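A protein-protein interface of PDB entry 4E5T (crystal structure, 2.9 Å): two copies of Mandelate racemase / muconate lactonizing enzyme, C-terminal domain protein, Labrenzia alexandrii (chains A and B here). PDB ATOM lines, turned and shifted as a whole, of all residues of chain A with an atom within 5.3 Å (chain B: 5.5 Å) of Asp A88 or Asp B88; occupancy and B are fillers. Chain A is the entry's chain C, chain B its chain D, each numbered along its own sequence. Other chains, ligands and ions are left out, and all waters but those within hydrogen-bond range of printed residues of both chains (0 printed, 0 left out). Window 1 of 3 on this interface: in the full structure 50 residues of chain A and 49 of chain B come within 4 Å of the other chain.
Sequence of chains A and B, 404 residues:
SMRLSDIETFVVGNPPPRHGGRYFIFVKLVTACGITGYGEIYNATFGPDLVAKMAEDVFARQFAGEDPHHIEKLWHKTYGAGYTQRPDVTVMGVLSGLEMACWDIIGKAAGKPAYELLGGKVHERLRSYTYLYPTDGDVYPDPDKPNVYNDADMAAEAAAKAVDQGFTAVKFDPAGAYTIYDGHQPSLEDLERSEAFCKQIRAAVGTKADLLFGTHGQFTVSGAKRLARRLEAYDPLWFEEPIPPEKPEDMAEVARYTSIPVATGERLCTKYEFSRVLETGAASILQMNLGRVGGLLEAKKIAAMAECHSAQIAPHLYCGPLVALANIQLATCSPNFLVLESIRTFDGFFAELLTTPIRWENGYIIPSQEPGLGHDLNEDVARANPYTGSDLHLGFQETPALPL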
ATOM      1  N   THR A  45      19.836 -24.343  31.778  1.00  0.00           N
ATOM      2  CA  THR A  45      19.019 -24.712  30.623  1.00  0.00           C
ATOM      3  C   THR A  45      19.730 -25.772  29.779  1.00  0.00           C
ATOM      4  O   THR A  45      19.151 -26.294  28.815  1.00  0.00           O
ATOM      5  CB  THR A  45      18.607 -23.481  29.740  1.00  0.00           C
ATOM      6  OG1 THR A  45      19.725 -22.604  29.553  1.00  0.00           O
ATOM      7  CG2 THR A  45      17.469 -22.702  30.373  1.00  0.00           C
ATOM      8  N   ARG A  86      16.533  -9.411  23.298  1.00  0.00           N
ATOM      9  CA  ARG A  86      15.303  -9.772  23.985  1.00  0.00           C
ATOM     10  C   ARG A  86      15.694 -10.612  25.189  1.00  0.00           C
ATOM     11  O   ARG A  86      16.714 -11.305  25.161  1.00  0.00           O
ATOM     12  CB  ARG A  86      14.366 -10.545  23.053  1.00  0.00           C
ATOM     13  CG  ARG A  86      15.023 -11.774  22.467  1.00  0.00           C
ATOM     14  CD  ARG A  86      14.040 -12.784  21.912  1.00  0.00           C
ATOM     15  NE  ARG A  86      12.823 -13.032  22.699  1.00  0.00           N
ATOM     16  CZ  ARG A  86      12.802 -13.503  23.940  1.00  0.00           C
ATOM     17  NH1 ARG A  86      13.927 -13.758  24.584  1.00  0.00           N
ATOM     18  NH2 ARG A  86      11.651 -13.694  24.558  1.00  0.00           N
ATOM     19  N   PRO A  87      14.908 -10.529  26.269  1.00  0.00           N
ATOM     20  CA  PRO A  87      15.293 -11.277  27.467  1.00  0.00           C
ATOM     21  C   PRO A  87      15.435 -12.759  27.140  1.00  0.00           C
ATOM     22  O   PRO A  87      14.468 -13.421  26.750  1.00  0.00           O
ATOM     23  CB  PRO A  87      14.112 -11.061  28.416  1.00  0.00           C
ATOM     24  CG  PRO A  87      13.375  -9.892  27.878  1.00  0.00           C
ATOM     25  CD  PRO A  87      13.599  -9.873  26.410  1.00  0.00           C
ATOM     26  N   ASP A  88      16.656 -13.258  27.258  1.00  0.00           N
ATOM     27  CA  ASP A  88      16.925 -14.673  27.079  1.00  0.00           C
ATOM     28  C   ASP A  88      17.673 -15.160  28.320  1.00  0.00           C
ATOM     29  O   ASP A  88      18.705 -14.600  28.661  1.00  0.00           O
ATOM     30  CB  ASP A  88      17.771 -14.858  25.815  1.00  0.00           C
ATOM     31  CG  ASP A  88      18.155 -16.309  25.558  1.00  0.00           C
ATOM     32  OD1 ASP A  88      17.325 -17.043  24.975  1.00  0.00           O
ATOM     33  OD2 ASP A  88      19.289 -16.705  25.922  1.00  0.00           O
ATOM     34  N   VAL A  89      17.168 -16.173  29.019  1.00  0.00           N
ATOM     35  CA  VAL A  89      17.865 -16.610  30.243  1.00  0.00           C
ATOM     36  C   VAL A  89      19.215 -17.281  29.990  1.00  0.00           C
ATOM     37  O   VAL A  89      20.150 -17.139  30.793  1.00  0.00           O
ATOM     38  CB  VAL A  89      17.022 -17.529  31.168  1.00  0.00           C
ATOM     39  CG1 VAL A  89      16.564 -16.763  32.391  1.00  0.00           C
ATOM     40  CG2 VAL A  89      15.861 -18.126  30.428  1.00  0.00           C
ATOM     41  N   THR A  90      19.315 -18.018  28.890  1.00  0.00           N
ATOM     42  CA  THR A  90      20.568 -18.666  28.571  1.00  0.00           C
ATOM     43  C   THR A  90      21.648 -17.595  28.424  1.00  0.00           C
ATOM     44  O   THR A  90      22.640 -17.628  29.144  1.00  0.00           O
ATOM     45  CB  THR A  90      20.474 -19.581  27.311  1.00  0.00           C
ATOM     46  OG1 THR A  90      19.343 -20.457  27.423  1.00  0.00           O
ATOM     47  CG2 THR A  90      21.733 -20.426  27.162  1.00  0.00           C
ATOM     48  N   VAL A  91      21.439 -16.629  27.531  1.00  0.00           N
ATOM     49  CA  VAL A  91      22.450 -15.599  27.307  1.00  0.00           C
ATOM     50  C   VAL A  91      22.713 -14.774  28.568  1.00  0.00           C
ATOM     51  O   VAL A  91      23.863 -14.594  28.988  1.00  0.00           O
ATOM     52  CB  VAL A  91      22.089 -14.636  26.153  1.00  0.00           C
ATOM     53  CG1 VAL A  91      23.117 -13.513  26.072  1.00  0.00           C
ATOM     54  CG2 VAL A  91      22.031 -15.366  24.829  1.00  0.00           C
ATOM     55  N   MET A  92      21.635 -14.294  29.177  1.00  0.00           N
ATOM     56  CA  MET A  92      21.729 -13.365  30.284  1.00  0.00           C
ATOM     57  C   MET A  92      22.471 -13.959  31.464  1.00  0.00           C
ATOM     58  O   MET A  92      23.204 -13.246  32.156  1.00  0.00           O
ATOM     59  CB  MET A  92      20.346 -12.876  30.696  1.00  0.00           C
ATOM     60  CG  MET A  92      20.301 -11.386  30.961  1.00  0.00           C
ATOM     61  SD  MET A  92      20.859 -10.390  29.574  1.00  0.00           S
ATOM     62  CE  MET A  92      19.792 -10.999  28.270  1.00  0.00           C
ATOM     63  N   GLY A  93      22.306 -15.264  31.671  1.00  0.00           N
ATOM     64  CA  GLY A  93      23.023 -15.969  32.725  1.00  0.00           C
ATOM     65  C   GLY A  93      24.528 -15.961  32.501  1.00  0.00           C
ATOM     66  O   GLY A  93      25.312 -15.945  33.455  1.00  0.00           O
ATOM     67  N   CYS A 269      14.950 -11.852  33.781  1.00  0.00           N
ATOM     68  CA  CYS A 269      16.209 -11.179  33.447  1.00  0.00           C
ATOM     69  C   CYS A 269      15.984  -9.898  32.672  1.00  0.00           C
ATOM     70  O   CYS A 269      14.944  -9.733  32.062  1.00  0.00           O
ATOM     71  CB  CYS A 269      17.162 -12.102  32.684  1.00  0.00           C
ATOM     72  SG  CYS A 269      16.541 -12.761  31.133  1.00  0.00           S
ATOM     73  N   THR B  45      22.346 -16.798  18.878  1.00  0.00           N
ATOM     74  CA  THR B  45      22.925 -16.267  20.107  1.00  0.00           C
ATOM     75  C   THR B  45      24.354 -16.797  20.282  1.00  0.00           C
ATOM     76  O   THR B  45      25.243 -16.092  20.766  1.00  0.00           O
ATOM     77  CB  THR B  45      22.076 -16.593  21.360  1.00  0.00           C
ATOM     78  OG1 THR B  45      21.693 -17.972  21.344  1.00  0.00           O
ATOM     79  CG2 THR B  45      20.829 -15.737  21.401  1.00  0.00           C
ATOM     80  N   PHE B  46      24.573 -18.041  19.868  1.00  0.00           N
ATOM     81  CA  PHE B  46      25.889 -18.654  19.971  1.00  0.00           C
ATOM     82  C   PHE B  46      26.265 -19.156  18.594  1.00  0.00           C
ATOM     83  O   PHE B  46      25.402 -19.265  17.721  1.00  0.00           O
ATOM     84  CB  PHE B  46      25.888 -19.799  21.001  1.00  0.00           C
ATOM     85  CG  PHE B  46      25.485 -19.362  22.394  1.00  0.00           C
ATOM     86  CD1 PHE B  46      26.408 -18.772  23.250  1.00  0.00           C
ATOM     87  CD2 PHE B  46      24.183 -19.523  22.842  1.00  0.00           C
ATOM     88  CE1 PHE B  46      26.041 -18.364  24.522  1.00  0.00           C
ATOM     89  CE2 PHE B  46      23.814 -19.116  24.118  1.00  0.00           C
ATOM     90  CZ  PHE B  46      24.749 -18.538  24.958  1.00  0.00           C
ATOM     91  N   ARG B  86      10.136 -20.087  30.974  1.00  0.00           N
ATOM     92  CA  ARG B  86       9.817 -18.756  30.455  1.00  0.00           C
ATOM     93  C   ARG B  86      10.597 -18.603  29.161  1.00  0.00           C
ATOM     94  O   ARG B  86      11.691 -19.142  29.030  1.00  0.00           O
ATOM     95  CB  ARG B  86      10.148 -17.637  31.456  1.00  0.00           C
ATOM     96  CG  ARG B  86      11.365 -17.874  32.353  1.00  0.00           C
ATOM     97  CD  ARG B  86      12.673 -17.417  31.718  1.00  0.00           C
ATOM     98  NE  ARG B  86      12.466 -16.609  30.521  1.00  0.00           N
ATOM     99  CZ  ARG B  86      12.735 -15.308  30.443  1.00  0.00           C
ATOM    100  NH1 ARG B  86      13.247 -14.659  31.485  1.00  0.00           N
ATOM    101  NH2 ARG B  86      12.496 -14.646  29.322  1.00  0.00           N
ATOM    102  N   PRO B  87      10.020 -17.908  28.183  1.00  0.00           N
ATOM    103  CA  PRO B  87      10.622 -17.802  26.856  1.00  0.00           C
ATOM    104  C   PRO B  87      12.116 -17.547  26.895  1.00  0.00           C
ATOM    105  O   PRO B  87      12.627 -16.902  27.797  1.00  0.00           O
ATOM    106  CB  PRO B  87       9.892 -16.609  26.260  1.00  0.00           C
ATOM    107  CG  PRO B  87       8.522 -16.753  26.813  1.00  0.00           C
ATOM    108  CD  PRO B  87       8.718 -17.230  28.239  1.00  0.00           C
ATOM    109  N   ASP B  88      12.811 -18.078  25.909  1.00  0.00           N
ATOM    110  CA  ASP B  88      14.255 -18.025  25.874  1.00  0.00           C
ATOM    111  C   ASP B  88      14.606 -18.522  24.492  1.00  0.00           C
ATOM    112  O   ASP B  88      14.585 -19.727  24.263  1.00  0.00           O
ATOM    113  CB  ASP B  88      14.806 -18.956  26.954  1.00  0.00           C
ATOM    114  CG  ASP B  88      16.302 -19.143  26.872  1.00  0.00           C
ATOM    115  OD1 ASP B  88      16.750 -20.027  26.119  1.00  0.00           O
ATOM    116  OD2 ASP B  88      17.039 -18.424  27.572  1.00  0.00           O
ATOM    117  N   VAL B  89      14.873 -17.607  23.560  1.00  0.00           N
ATOM    118  CA  VAL B  89      15.091 -18.013  22.166  1.00  0.00           C
ATOM    119  C   VAL B  89      16.109 -19.135  22.032  1.00  0.00           C
ATOM    120  O   VAL B  89      15.872 -20.074  21.292  1.00  0.00           O
ATOM    121  CB  VAL B  89      15.472 -16.850  21.213  1.00  0.00           C
ATOM    122  CG1 VAL B  89      14.239 -16.125  20.762  1.00  0.00           C
ATOM    123  CG2 VAL B  89      16.446 -15.924  21.847  1.00  0.00           C
ATOM    124  N   THR B  90      17.214 -19.043  22.770  1.00  0.00           N
ATOM    125  CA  THR B  90      18.260 -20.071  22.767  1.00  0.00           C
ATOM    126  C   THR B  90      17.710 -21.503  22.882  1.00  0.00           C
ATOM    127  O   THR B  90      17.984 -22.345  22.016  1.00  0.00           O
ATOM    128  CB  THR B  90      19.316 -19.824  23.874  1.00  0.00           C
ATOM    129  OG1 THR B  90      19.925 -18.542  23.687  1.00  0.00           O
ATOM    130  CG2 THR B  90      20.391 -20.872  23.817  1.00  0.00           C
ATOM    131  N   VAL B  91      16.929 -21.769  23.931  1.00  0.00           N
ATOM    132  CA  VAL B  91      16.301 -23.077  24.115  1.00  0.00           C
ATOM    133  C   VAL B  91      15.205 -23.329  23.083  1.00  0.00           C
ATOM    134  O   VAL B  91      15.243 -24.314  22.340  1.00  0.00           O
ATOM    135  CB  VAL B  91      15.669 -23.215  25.506  1.00  0.00           C
ATOM    136  CG1 VAL B  91      14.932 -24.544  25.625  1.00  0.00           C
ATOM    137  CG2 VAL B  91      16.719 -23.086  26.591  1.00  0.00           C
ATOM    138  N   MET B  92      14.228 -22.427  23.062  1.00  0.00           N
ATOM    139  CA  MET B  92      13.088 -22.462  22.146  1.00  0.00           C
ATOM    140  C   MET B  92      13.461 -22.715  20.674  1.00  0.00           C
ATOM    141  O   MET B  92      12.696 -23.317  19.932  1.00  0.00           O
ATOM    142  CB  MET B  92      12.318 -21.146  22.281  1.00  0.00           C
ATOM    143  CG  MET B  92      10.844 -21.273  22.595  1.00  0.00           C
ATOM    144  SD  MET B  92      10.323 -22.850  23.251  1.00  0.00           S
ATOM    145  CE  MET B  92      10.990 -22.790  24.907  1.00  0.00           C
ATOM    146  N   GLY B  93      14.634 -22.250  20.254  1.00  0.00           N
ATOM    147  CA  GLY B  93      15.134 -22.526  18.919  1.00  0.00           C
ATOM    148  C   GLY B  93      15.416 -24.011  18.749  1.00  0.00           C
ATOM    149  O   GLY B  93      14.922 -24.652  17.822  1.00  0.00           O
ATOM    150  N   CYS B 269       8.972 -15.916  20.806  1.00  0.00           N
ATOM    151  CA  CYS B 269       8.751 -17.354  20.925  1.00  0.00           C
ATOM    152  C   CYS B 269       7.692 -17.717  21.962  1.00  0.00           C
ATOM    153  O   CYS B 269       7.428 -16.957  22.884  1.00  0.00           O
ATOM    154  CB  CYS B 269      10.061 -18.093  21.223  1.00  0.00           C
ATOM    155  SG  CYS B 269      10.963 -17.598  22.714  1.00  0.00           S
ATOM    156  N   THR B 270       7.117 -18.907  21.802  1.00  0.00           N
ATOM    157  CA  THR B 270       6.052 -19.455  22.657  1.00  0.00           C
ATOM    158  C   THR B 270       4.750 -18.677  22.567  1.00  0.00           C
ATOM    159  O   THR B 270       4.752 -17.471  22.336  1.00  0.00           O
ATOM    160  CB  THR B 270       6.433 -19.534  24.127  1.00  0.00           C
ATOM    161  OG1 THR B 270       6.114 -18.290  24.739  1.00  0.00           O
ATOM    162  CG2 THR B 270       7.927 -19.844  24.308  1.00  0.00           C
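O of Pro A87 sits at hydrogen-bond distance from NH2 of Arg B86 (3.5 Å).
OD1 of Asp A88 lies within hydrogen-bond range of N of Val B89, 2.9 Å away.
The side-chain carboxylate (OD2) of Asp A88 sits at hydrogen-bond distance from the side-chain hydroxyl (OG1) of Thr B90 (3.0 Å).
The backbone NH (N) of Val A89 sits at hydrogen-bond distance from the side-chain carboxylate (OD2) of Asp B88 (2.7 Å).
N of Thr A90 sits at hydrogen-bond distance from OD2 of Asp B88.
The side-chain carboxylate (OD1) of Asp A88 sits close to the side-chain carboxylate (OD2) of Asp B88 (3.0 Å).
The side-chain hydroxyl (OG1) of Thr A90 is in hydrogen-bond range of the side-chain hydroxyl (OG1) of Thr A45 (3.0 Å).
The backbone NH (N) of Thr A90 sits at hydrogen-bond distance from the side-chain carboxylate (OD2) of Asp A88 (3.2 Å).
The backbone NH of Val A91 lies within hydrogen-bond range of the side-chain carboxylate of Asp A88 (2.7 Å).
The backbone carbonyl oxygen (O) of Asp A88 lies within hydrogen-bond range of the side-chain sulfur (SG) of Cys A269, 3.8 Å away.
The side-chain hydroxyl of Thr B90 is in hydrogen-bond range of the side-chain hydroxyl of Thr B45 (3.0 Å).
The side-chain sulfur of Cys B269 lies within hydrogen-bond range of the backbone NH of Asp B88, 3.7 Å away.
Among the printed residues, pairs that only touch across the chains: Val A89 with Arg B86 (3.5 Å), Arg A86 with Val B89 (3.5 Å), Thr A90 with Thr B90 (3.6 Å), Val A91 with Thr B45 (3.7 Å), Thr A45 with Val B91 (3.7 Å), Arg A86 with Pro B87 (3.8 Å), Thr A90 with Val B91 (3.8 Å), Cys A269 with Arg B86 (3.8 Å), Thr A90 with Phe B46 (3.9 Å) and Val A91 with Thr B90 (3.98 Å).
Of the printed residues of chain B, Pro A87 touches Arg B86.
Asp A88 touches just these residues of chain B: Asp B88 (3.0 Å), Val B89 (2.9 Å) and Thr B90 (3.0 Å).
Of the printed residues of chain B, Val A91 touches Thr B45 and Thr B90.
Of chain A, only Asp A88 (3.0 Å), Val A89 (2.7 Å) and Thr A90 (2.7 Å) come within 4 Å of Asp B88.
Of the printed residues of chain A, Val B89 touches Arg A86 (3.5 Å) and Asp A88 (2.9 Å).
The nearest printed residue of chain A that does not touch Thr B90 is Thr A45 (6.0 Å).
Of the 10 printed residues of chain A, 8 touch a printed residue of chain B.
Printed residues of chain A that touch a printed residue of chain B: Thr A45, Arg A86, Pro A87, Asp A88, Val A89, Thr A90, Val A91 and Cys A269.
Hydrophobic or aromatic side chains of chain B within 4 Å of the printed part of chain A: Phe B46, Pro B87, Val B89 and Val B91.
Among the printed residues, 16 pairs touch across the chains.
Among the printed residues, no Asp or Glu carboxylate lies within 4 Å of a Lys or Arg side-chain nitrogen of the other chain.
Thr A45 touches Val B91, and with the chains exchanged Val A91 touches Thr B45.
Asp B88 touches its own counterpart, Asp A88.
Thr B90 touches its own counterpart, Thr A90.
Thr A90 touches Val B91, and with the chains exchanged Val A91 touches Thr B90.
Positions printed for both chains: 45, 86, 87, 88, 89, 90, 91, 92, 93 and 269.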
